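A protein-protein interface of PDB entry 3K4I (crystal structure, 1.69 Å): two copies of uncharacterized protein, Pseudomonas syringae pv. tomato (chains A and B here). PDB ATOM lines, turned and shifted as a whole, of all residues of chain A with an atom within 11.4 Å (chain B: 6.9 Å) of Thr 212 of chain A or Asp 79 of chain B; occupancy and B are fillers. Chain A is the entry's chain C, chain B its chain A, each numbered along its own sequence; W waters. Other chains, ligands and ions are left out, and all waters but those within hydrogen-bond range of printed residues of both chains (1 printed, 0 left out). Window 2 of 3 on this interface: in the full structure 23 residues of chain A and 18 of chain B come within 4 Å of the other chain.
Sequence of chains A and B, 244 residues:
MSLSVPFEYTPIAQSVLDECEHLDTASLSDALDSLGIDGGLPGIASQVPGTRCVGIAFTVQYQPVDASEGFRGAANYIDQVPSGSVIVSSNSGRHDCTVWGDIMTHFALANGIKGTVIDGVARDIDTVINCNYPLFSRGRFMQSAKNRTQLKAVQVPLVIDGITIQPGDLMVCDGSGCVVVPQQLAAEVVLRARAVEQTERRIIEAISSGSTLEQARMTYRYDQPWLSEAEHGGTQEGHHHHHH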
ATOM      1  N   THR A 199       1.323  16.603  18.736  1.00  0.00           N
ATOM      2  CA  THR A 199       1.403  17.328  17.452  1.00  0.00           C
ATOM      3  C   THR A 199       1.361  18.842  17.664  1.00  0.00           C
ATOM      4  O   THR A 199       2.155  19.594  17.075  1.00  0.00           O
ATOM      5  CB  THR A 199       0.277  16.895  16.472  1.00  0.00           C
ATOM      6  OG1 THR A 199       0.462  15.519  16.118  1.00  0.00           O
ATOM      7  CG2 THR A 199       0.310  17.742  15.208  1.00  0.00           C
ATOM      8  N   GLU A 200       0.451  19.284  18.524  1.00  0.00           N
ATOM      9  CA  GLU A 200       0.266  20.706  18.793  1.00  0.00           C
ATOM     10  C   GLU A 200       1.442  21.336  19.515  1.00  0.00           C
ATOM     11  O   GLU A 200       1.786  22.499  19.270  1.00  0.00           O
ATOM     12  CB  GLU A 200      -0.947  20.923  19.666  1.00  0.00           C
ATOM     13  CG  GLU A 200      -2.242  20.943  18.966  1.00  0.00           C
ATOM     14  CD  GLU A 200      -3.317  21.487  19.876  1.00  0.00           C
ATOM     15  OE1 GLU A 200      -2.973  22.094  20.947  1.00  0.00           O
ATOM     16  OE2 GLU A 200      -4.496  21.316  19.511  1.00  0.00           O
ATOM     17  N   ARG A 202       4.515  20.517  19.202  1.00  0.00           N
ATOM     18  CA  ARG A 202       5.578  20.742  18.217  1.00  0.00           C
ATOM     19  C   ARG A 202       5.230  21.964  17.368  1.00  0.00           C
ATOM     20  O   ARG A 202       6.089  22.770  17.046  1.00  0.00           O
ATOM     21  CB  ARG A 202       5.779  19.505  17.345  1.00  0.00           C
ATOM     22  CG  ARG A 202       6.263  18.276  18.109  1.00  0.00           C
ATOM     23  CD  ARG A 202       6.802  17.223  17.152  1.00  0.00           C
ATOM     24  NE  ARG A 202       5.745  16.488  16.455  1.00  0.00           N
ATOM     25  CZ  ARG A 202       5.295  15.285  16.814  1.00  0.00           C
ATOM     26  NH1 ARG A 202       4.332  14.702  16.105  1.00  0.00           N
ATOM     27  NH2 ARG A 202       5.807  14.662  17.880  1.00  0.00           N
ATOM     28  N   ILE A 203       3.945  22.126  17.043  1.00  0.00           N
ATOM     29  CA  ILE A 203       3.560  23.286  16.265  1.00  0.00           C
ATOM     30  C   ILE A 203       3.845  24.586  17.036  1.00  0.00           C
ATOM     31  O   ILE A 203       4.421  25.548  16.480  1.00  0.00           O
ATOM     32  CB  ILE A 203       2.092  23.198  15.772  1.00  0.00           C
ATOM     33  CG1 ILE A 203       1.973  22.156  14.652  1.00  0.00           C
ATOM     34  CG2 ILE A 203       1.628  24.573  15.273  1.00  0.00           C
ATOM     35  CD1 ILE A 203       0.506  21.766  14.339  1.00  0.00           C
ATOM     36  N   ILE A 204       3.463  24.595  18.310  1.00  0.00           N
ATOM     37  CA  ILE A 204       3.726  25.726  19.190  1.00  0.00           C
ATOM     38  C   ILE A 204       5.228  25.987  19.305  1.00  0.00           C
ATOM     39  O   ILE A 204       5.681  27.141  19.214  1.00  0.00           O
ATOM     40  CB  ILE A 204       3.096  25.483  20.565  1.00  0.00           C
ATOM     41  CG1 ILE A 204       1.579  25.740  20.490  1.00  0.00           C
ATOM     42  CG2 ILE A 204       3.759  26.367  21.643  1.00  0.00           C
ATOM     43  CD1 ILE A 204       0.737  25.155  21.688  1.00  0.00           C
ATOM     44  N   GLU A 205       5.981  24.919  19.513  1.00  0.00           N
ATOM     45  CA  GLU A 205       7.445  25.067  19.583  1.00  0.00           C
ATOM     46  C   GLU A 205       8.008  25.703  18.304  1.00  0.00           C
ATOM     47  O   GLU A 205       8.888  26.588  18.365  1.00  0.00           O
ATOM     48  CB  GLU A 205       8.097  23.739  19.901  1.00  0.00           C
ATOM     49  CG  GLU A 205       7.893  23.326  21.337  1.00  0.00           C
ATOM     50  CD  GLU A 205       8.090  21.833  21.581  1.00  0.00           C
ATOM     51  OE1 GLU A 205       8.431  21.071  20.638  1.00  0.00           O
ATOM     52  OE2 GLU A 205       7.863  21.420  22.742  1.00  0.00           O
ATOM     53  N   ALA A 206       7.464  25.288  17.159  1.00  0.00           N
ATOM     54  CA  ALA A 206       7.892  25.832  15.892  1.00  0.00           C
ATOM     55  C   ALA A 206       7.579  27.326  15.728  1.00  0.00           C
ATOM     56  O   ALA A 206       8.460  28.134  15.385  1.00  0.00           O
ATOM     57  CB  ALA A 206       7.302  24.989  14.718  1.00  0.00           C
ATOM     58  N   ILE A 207       6.320  27.700  15.939  1.00  0.00           N
ATOM     59  CA  ILE A 207       5.974  29.107  15.854  1.00  0.00           C
ATOM     60  C   ILE A 207       6.681  29.973  16.903  1.00  0.00           C
ATOM     61  O   ILE A 207       6.906  31.154  16.657  1.00  0.00           O
ATOM     62  CB  ILE A 207       4.452  29.370  15.812  1.00  0.00           C
ATOM     63  CG1 ILE A 207       3.785  28.995  17.140  1.00  0.00           C
ATOM     64  CG2 ILE A 207       3.838  28.652  14.594  1.00  0.00           C
ATOM     65  CD1 ILE A 207       2.251  29.045  17.070  1.00  0.00           C
ATOM     66  N   SER A 208       7.083  29.376  18.034  1.00  0.00           N
ATOM     67  CA  SER A 208       7.817  30.114  19.064  1.00  0.00           C
ATOM     68  C   SER A 208       9.323  30.214  18.745  1.00  0.00           C
ATOM     69  O   SER A 208      10.098  30.866  19.468  1.00  0.00           O
ATOM     70  CB  SER A 208       7.569  29.484  20.450  1.00  0.00           C
ATOM     71  OG  SER A 208       6.215  29.685  20.881  1.00  0.00           O
ATOM     72  N   SER A 209       9.716  29.564  17.656  1.00  0.00           N
ATOM     73  CA  SER A 209      11.064  29.683  17.131  1.00  0.00           C
ATOM     74  C   SER A 209      11.093  30.425  15.788  1.00  0.00           C
ATOM     75  O   SER A 209      12.090  30.383  15.068  1.00  0.00           O
ATOM     76  CB  SER A 209      11.756  28.299  17.085  1.00  0.00           C
ATOM     77  OG  SER A 209      11.076  27.401  16.207  1.00  0.00           O
ATOM     78  N   GLY A 210       9.985  31.111  15.470  1.00  0.00           N
ATOM     79  CA  GLY A 210       9.922  31.979  14.293  1.00  0.00           C
ATOM     80  C   GLY A 210       9.419  31.342  13.012  1.00  0.00           C
ATOM     81  O   GLY A 210       9.532  31.943  11.948  1.00  0.00           O
ATOM     82  N   SER A 211       8.846  30.143  13.098  1.00  0.00           N
ATOM     83  CA  SER A 211       8.161  29.549  11.950  1.00  0.00           C
ATOM     84  C   SER A 211       6.896  30.321  11.683  1.00  0.00           C
ATOM     85  O   SER A 211       6.239  30.756  12.628  1.00  0.00           O
ATOM     86  CB  SER A 211       7.736  28.120  12.273  1.00  0.00           C
ATOM     87  OG  SER A 211       7.061  27.503  11.181  1.00  0.00           O
ATOM     88  N   THR A 212       6.526  30.449  10.407  1.00  0.00           N
ATOM     89  CA  THR A 212       5.123  30.817  10.104  1.00  0.00           C
ATOM     90  C   THR A 212       4.233  29.655  10.542  1.00  0.00           C
ATOM     91  O   THR A 212       4.689  28.505  10.673  1.00  0.00           O
ATOM     92  CB  THR A 212       4.877  31.049   8.590  1.00  0.00           C
ATOM     93  OG1 THR A 212       5.120  29.838   7.860  1.00  0.00           O
ATOM     94  CG2 THR A 212       5.744  32.159   8.047  1.00  0.00           C
ATOM     95  N   LEU A 213       2.952  29.947  10.781  1.00  0.00           N
ATOM     96  CA  LEU A 213       2.009  28.906  11.117  1.00  0.00           C
ATOM     97  C   LEU A 213       1.872  27.945   9.931  1.00  0.00           C
ATOM     98  O   LEU A 213       1.802  26.718  10.118  1.00  0.00           O
ATOM     99  CB  LEU A 213       0.655  29.504  11.532  1.00  0.00           C
ATOM    100  CG  LEU A 213      -0.427  28.535  12.049  1.00  0.00           C
ATOM    101  CD1 LEU A 213       0.163  27.584  13.094  1.00  0.00           C
ATOM    102  CD2 LEU A 213      -1.606  29.289  12.646  1.00  0.00           C
ATOM    103  N   GLU A 214       1.870  28.508   8.717  1.00  0.00           N
ATOM    104  CA  GLU A 214       1.795  27.713   7.489  1.00  0.00           C
ATOM    105  C   GLU A 214       2.867  26.628   7.496  1.00  0.00           C
ATOM    106  O   GLU A 214       2.548  25.446   7.332  1.00  0.00           O
ATOM    107  CB  GLU A 214       1.985  28.591   6.255  1.00  0.00           C
ATOM    108  CG  GLU A 214       0.730  29.318   5.814  1.00  0.00           C
ATOM    109  CD  GLU A 214       0.728  29.656   4.326  1.00  0.00           C
ATOM    110  OE1 GLU A 214      -0.255  30.294   3.882  1.00  0.00           O
ATOM    111  OE2 GLU A 214       1.691  29.287   3.606  1.00  0.00           O
ATOM    112  N   GLN A 215       4.117  27.047   7.711  1.00  0.00           N
ATOM    113  CA  GLN A 215       5.289  26.145   7.753  1.00  0.00           C
ATOM    114  C   GLN A 215       5.125  25.048   8.793  1.00  0.00           C
ATOM    115  O   GLN A 215       5.312  23.860   8.497  1.00  0.00           O
ATOM    116  CB  GLN A 215       6.553  26.907   8.132  1.00  0.00           C
ATOM    117  CG  GLN A 215       7.151  27.861   7.137  1.00  0.00           C
ATOM    118  CD  GLN A 215       8.465  28.418   7.669  1.00  0.00           C
ATOM    119  OE1 GLN A 215       8.508  29.483   8.315  1.00  0.00           O
ATOM    120  NE2 GLN A 215       9.547  27.666   7.445  1.00  0.00           N
ATOM    121  N   ALA A 216       4.800  25.466  10.019  1.00  0.00           N
ATOM    122  CA  ALA A 216       4.651  24.559  11.153  1.00  0.00           C
ATOM    123  C   ALA A 216       3.595  23.483  10.911  1.00  0.00           C
ATOM    124  O   ALA A 216       3.824  22.310  11.196  1.00  0.00           O
ATOM    125  CB  ALA A 216       4.323  25.349  12.427  1.00  0.00           C
ATOM    126  N   ARG A 217       2.452  23.887  10.363  1.00  0.00           N
ATOM    127  CA  ARG A 217       1.303  22.983  10.174  1.00  0.00           C
ATOM    128  C   ARG A 217       1.533  21.818   9.201  1.00  0.00           C
ATOM    129  O   ARG A 217       0.896  20.768   9.318  1.00  0.00           O
ATOM    130  CB  ARG A 217       0.048  23.773   9.784  1.00  0.00           C
ATOM    131  CG  ARG A 217      -0.656  24.396  10.967  1.00  0.00           C
ATOM    132  CD  ARG A 217      -1.885  25.183  10.552  1.00  0.00           C
ATOM    133  NE  ARG A 217      -2.634  25.610  11.732  1.00  0.00           N
ATOM    134  CZ  ARG A 217      -3.710  26.391  11.718  1.00  0.00           C
ATOM    135  NH1 ARG A 217      -4.193  26.867  10.572  1.00  0.00           N
ATOM    136  NH2 ARG A 217      -4.301  26.709  12.864  1.00  0.00           N
ATOM    137  N   MET A 218       2.431  21.994   8.243  1.00  0.00           N
ATOM    138  CA  MET A 218       2.710  20.898   7.322  1.00  0.00           C
ATOM    139  C   MET A 218       4.108  20.314   7.454  1.00  0.00           C
ATOM    140  O   MET A 218       4.490  19.433   6.684  1.00  0.00           O
ATOM    141  CB  MET A 218       2.392  21.275   5.878  1.00  0.00           C
ATOM    142  CG  MET A 218       2.161  22.737   5.658  1.00  0.00           C
ATOM    143  SD  MET A 218       2.411  23.156   3.792  1.00  0.00           S
ATOM    144  CE  MET A 218       4.230  23.888   3.869  1.00  0.00           C
ATOM    145  N   THR A 219       4.876  20.796   8.421  1.00  0.00           N
ATOM    146  CA  THR A 219       6.038  20.029   8.854  1.00  0.00           C
ATOM    147  C   THR A 219       5.587  19.082   9.973  1.00  0.00           C
ATOM    148  O   THR A 219       6.269  18.094  10.272  1.00  0.00           O
ATOM    149  CB  THR A 219       7.248  20.914   9.254  1.00  0.00           C
ATOM    150  OG1 THR A 219       6.842  21.905  10.198  1.00  0.00           O
ATOM    151  CG2 THR A 219       7.833  21.613   8.035  1.00  0.00           C
ATOM    152  N   TYR A 220       4.420  19.388  10.558  1.00  0.00           N
ATOM    153  CA  TYR A 220       3.777  18.572  11.605  1.00  0.00           C
ATOM    154  C   TYR A 220       2.279  18.424  11.340  1.00  0.00           C
ATOM    155  O   TYR A 220       1.776  17.317  11.140  1.00  0.00           O
ATOM    156  CB  TYR A 220       4.002  19.181  12.998  1.00  0.00           C
ATOM    157  CG  TYR A 220       5.451  19.511  13.266  1.00  0.00           C
ATOM    158  CD1 TYR A 220       5.921  20.816  13.139  1.00  0.00           C
ATOM    159  CD2 TYR A 220       6.360  18.511  13.612  1.00  0.00           C
ATOM    160  CE1 TYR A 220       7.253  21.126  13.363  1.00  0.00           C
ATOM    161  CE2 TYR A 220       7.700  18.811  13.838  1.00  0.00           C
ATOM    162  CZ  TYR A 220       8.137  20.118  13.709  1.00  0.00           C
ATOM    163  OH  TYR A 220       9.456  20.415  13.928  1.00  0.00           O
ATOM    164  N   ASN B  76      -3.055  29.219   8.789  1.00  0.00           N
ATOM    165  CA  ASN B  76      -4.206  30.003   8.306  1.00  0.00           C
ATOM    166  C   ASN B  76      -3.878  31.498   8.136  1.00  0.00           C
ATOM    167  O   ASN B  76      -2.727  31.869   7.855  1.00  0.00           O
ATOM    168  CB  ASN B  76      -5.472  29.777   9.178  1.00  0.00           C
ATOM    169  CG  ASN B  76      -5.299  30.186  10.668  1.00  0.00           C
ATOM    170  OD1 ASN B  76      -6.040  29.696  11.538  1.00  0.00           O
ATOM    171  ND2 ASN B  76      -4.360  31.095  10.958  1.00  0.00           N
ATOM    172  N   TYR B  77      -4.880  32.342   8.344  1.00  0.00           N
ATOM    173  CA  TYR B  77      -4.770  33.784   8.114  1.00  0.00           C
ATOM    174  C   TYR B  77      -3.698  34.492   8.960  1.00  0.00           C
ATOM    175  O   TYR B  77      -3.242  35.589   8.607  1.00  0.00           O
ATOM    176  CB  TYR B  77      -6.120  34.453   8.420  1.00  0.00           C
ATOM    177  CG  TYR B  77      -6.436  34.559   9.905  1.00  0.00           C
ATOM    178  CD1 TYR B  77      -7.119  33.534  10.576  1.00  0.00           C
ATOM    179  CD2 TYR B  77      -6.024  35.678  10.652  1.00  0.00           C
ATOM    180  CE1 TYR B  77      -7.395  33.628  11.950  1.00  0.00           C
ATOM    181  CE2 TYR B  77      -6.289  35.773  12.016  1.00  0.00           C
ATOM    182  CZ  TYR B  77      -6.962  34.747  12.659  1.00  0.00           C
ATOM    183  OH  TYR B  77      -7.208  34.896  14.017  1.00  0.00           O
ATOM    184  N   ILE B  78      -3.345  33.895  10.090  1.00  0.00           N
ATOM    185  CA  ILE B  78      -2.627  34.656  11.136  1.00  0.00           C
ATOM    186  C   ILE B  78      -1.221  35.098  10.685  1.00  0.00           C
ATOM    187  O   ILE B  78      -0.693  36.093  11.182  1.00  0.00           O
ATOM    188  CB  ILE B  78      -2.641  33.937  12.516  1.00  0.00           C
ATOM    189  CG1 ILE B  78      -2.411  34.934  13.663  1.00  0.00           C
ATOM    190  CG2 ILE B  78      -1.665  32.777  12.532  1.00  0.00           C
ATOM    191  CD1 ILE B  78      -2.686  34.394  15.038  1.00  0.00           C
ATOM    192  N   ASP B  79      -0.664  34.405   9.694  1.00  0.00           N
ATOM    193  CA  ASP B  79       0.639  34.790   9.150  1.00  0.00           C
ATOM    194  C   ASP B  79       0.633  36.165   8.497  1.00  0.00           C
ATOM    195  O   ASP B  79       1.691  36.796   8.338  1.00  0.00           O
ATOM    196  CB  ASP B  79       1.141  33.745   8.150  1.00  0.00           C
ATOM    197  CG  ASP B  79       1.599  32.457   8.830  1.00  0.00           C
ATOM    198  OD1 ASP B  79       2.249  32.565   9.896  1.00  0.00           O
ATOM    199  OD2 ASP B  79       1.337  31.352   8.298  1.00  0.00           O
ATOM    200  N   GLN B  80      -0.561  36.612   8.111  1.00  0.00           N
ATOM    201  CA  GLN B  80      -0.743  37.910   7.479  1.00  0.00           C
ATOM    202  C   GLN B  80      -0.995  39.069   8.449  1.00  0.00           C
ATOM    203  O   GLN B  80      -1.072  40.225   8.008  1.00  0.00           O
ATOM    204  CB  GLN B  80      -1.920  37.875   6.487  1.00  0.00           C
ATOM    205  CG  GLN B  80      -1.907  36.729   5.508  1.00  0.00           C
ATOM    206  CD  GLN B  80      -3.296  36.453   4.952  1.00  0.00           C
ATOM    207  OE1 GLN B  80      -3.718  35.296   4.878  1.00  0.00           O
ATOM    208  NE2 GLN B  80      -4.022  37.515   4.582  1.00  0.00           N
ATOM    209  N   VAL B  81      -1.102  38.790   9.751  1.00  0.00           N
ATOM    210  CA  VAL B  81      -1.448  39.841  10.705  1.00  0.00           C
ATOM    211  C   VAL B  81      -0.196  40.646  11.129  1.00  0.00           C
ATOM    212  O   VAL B  81       0.750  40.070  11.688  1.00  0.00           O
ATOM    213  CB  VAL B  81      -2.159  39.252  11.947  1.00  0.00           C
ATOM    214  CG1 VAL B  81      -2.440  40.345  12.997  1.00  0.00           C
ATOM    215  CG2 VAL B  81      -3.456  38.535  11.538  1.00  0.00           C
ATOM    216  N   PRO B  82      -0.175  41.963  10.854  1.00  0.00           N
ATOM    217  CA  PRO B  82       0.983  42.784  11.233  1.00  0.00           C
ATOM    218  C   PRO B  82       1.143  42.915  12.736  1.00  0.00           C
ATOM    219  O   PRO B  82       0.155  42.951  13.462  1.00  0.00           O
ATOM    220  CB  PRO B  82       0.632  44.170  10.659  1.00  0.00           C
ATOM    221  CG  PRO B  82      -0.368  43.890   9.578  1.00  0.00           C
ATOM    222  CD  PRO B  82      -1.189  42.774  10.154  1.00  0.00           C
ATOM    223  N   PHE B 107       1.341  32.031  18.985  1.00  0.00           N
ATOM    224  CA  PHE B 107       1.665  32.815  17.775  1.00  0.00           C
ATOM    225  C   PHE B 107       1.640  34.343  18.035  1.00  0.00           C
ATOM    226  O   PHE B 107       2.553  35.118  17.656  1.00  0.00           O
ATOM    227  CB  PHE B 107       0.768  32.438  16.579  1.00  0.00           C
ATOM    228  CG  PHE B 107       1.220  33.088  15.292  1.00  0.00           C
ATOM    229  CD1 PHE B 107       2.080  32.426  14.419  1.00  0.00           C
ATOM    230  CD2 PHE B 107       0.867  34.419  15.014  1.00  0.00           C
ATOM    231  CE1 PHE B 107       2.554  33.058  13.247  1.00  0.00           C
ATOM    232  CE2 PHE B 107       1.331  35.056  13.869  1.00  0.00           C
ATOM    233  CZ  PHE B 107       2.181  34.384  12.986  1.00  0.00           C
ATOM    234  N   ASN B 111       4.753  37.280  17.756  1.00  0.00           N
ATOM    235  CA  ASN B 111       4.629  38.076  16.532  1.00  0.00           C
ATOM    236  C   ASN B 111       4.012  39.454  16.759  1.00  0.00           C
ATOM    237  O   ASN B 111       3.550  40.130  15.824  1.00  0.00           O
ATOM    238  CB  ASN B 111       3.853  37.256  15.501  1.00  0.00           C
ATOM    239  CG  ASN B 111       4.704  36.186  14.879  1.00  0.00           C
ATOM    240  OD1 ASN B 111       5.507  36.479  13.979  1.00  0.00           O
ATOM    241  ND2 ASN B 111       4.564  34.935  15.361  1.00  0.00           N
ATOM    242  N   ILE B 113       1.342  40.539  18.221  1.00  0.00           N
ATOM    243  CA  ILE B 113      -0.116  40.747  18.206  1.00  0.00           C
ATOM    244  C   ILE B 113      -0.599  41.053  19.640  1.00  0.00           C
ATOM    245  O   ILE B 113      -0.241  40.338  20.616  1.00  0.00           O
ATOM    246  CB  ILE B 113      -0.810  39.557  17.503  1.00  0.00           C
ATOM    247  CG1 ILE B 113      -0.362  39.504  16.036  1.00  0.00           C
ATOM    248  CG2 ILE B 113      -2.336  39.665  17.569  1.00  0.00           C
ATOM    249  CD1 ILE B 113      -0.559  38.141  15.356  1.00  0.00           C
HETATM  250  O   HOH W   1       6.178  32.811  14.630  1.00  0.00           O
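The backbone NH (N) of Ile 78 of chain B sits close to the side-chain amide nitrogen (ND2) of Asn 76 of chain B (3.1 Å).
The side-chain hydroxyl (OG1) of Thr 212 of chain A sits close to the backbone NH (N) of Gln 215 of chain A, at 3.0 Å.
O of Phe 107 of chain B is in hydrogen-bond range of ND2 of Asn 111 of chain B.
Of the 10 printed residues of chain B, 4 touch a printed residue of chain A.
Along chain B the printed residues that touch a printed residue of chain A span positions 76 to 107.
Among the printed residues, 8 pairs touch across the chains.
No position is printed for both chains.
Of the 8 pairs that touch across the chains among the printed residues, none has its exchanged pair printed and touching as well.
The side-chain carboxylate (OD1) of Asp 79 of chain B lies within hydrogen-bond range of the backbone NH (N) of Leu 213 of chain A (2.9 Å).
The side-chain carboxylate (OD2) of Asp 79 of chain B lies within hydrogen-bond range of the backbone NH (N) of Glu 214 of chain A (2.9 Å).
The guanidinium group (NH1) of Arg 217 of chain A lies close to the backbone NH (N) of Asn 76 of chain B, 3.2 Å away.
Water W1 lies within hydrogen-bond range of O of Ile 207 of chain A (2.7 Å), ND2 of Asn 111 of chain B (2.8 Å) and O of Ser 211 of chain A (2.9 Å).
Ile 207 of chain A touches Phe 107 of chain B.
Thr 212 of chain A touches Asp 79 of chain B.
ND2 of Asn 76 of chain B touches CD2 of Leu 213 of chain A, 3.7 Å away.
Ile 78 of chain B touches Leu 213 of chain A (CG2 to CD2, 3.5 Å).
Phe 107 of chain B touches Leu 213 of chain A (CE1 to N, 3.99 Å).
Arg 202 of chain A touches none of the printed residues of chain B.
Thr 212 of chain A touches just one residue of chain B: Asp 79 (3.3 Å).
Printed residues of chain B within 4 Å of Glu 214 of chain A: Asp 79 (2.9 Å).
Met 218 of chain A touches none of the printed residues of chain B.
Printed residues of chain A within 4 Å of Asp 79 of chain B: Thr 212 (3.3 Å), Leu 213 (2.9 Å) and Glu 214 (2.9 Å).
No residue of chain A comes within 4 Å of Gln 80 of chain B.
No residue of chain A comes within 4 Å of Val 81 of chain B.
Printed residues of chain A within 4 Å of Phe 107 of chain B: Ile 207 (3.7 Å) and Leu 213 (3.99 Å).
The nearest residue of chain B that does not touch Thr 212 of chain A is Phe 107 of chain B (4.6 Å).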
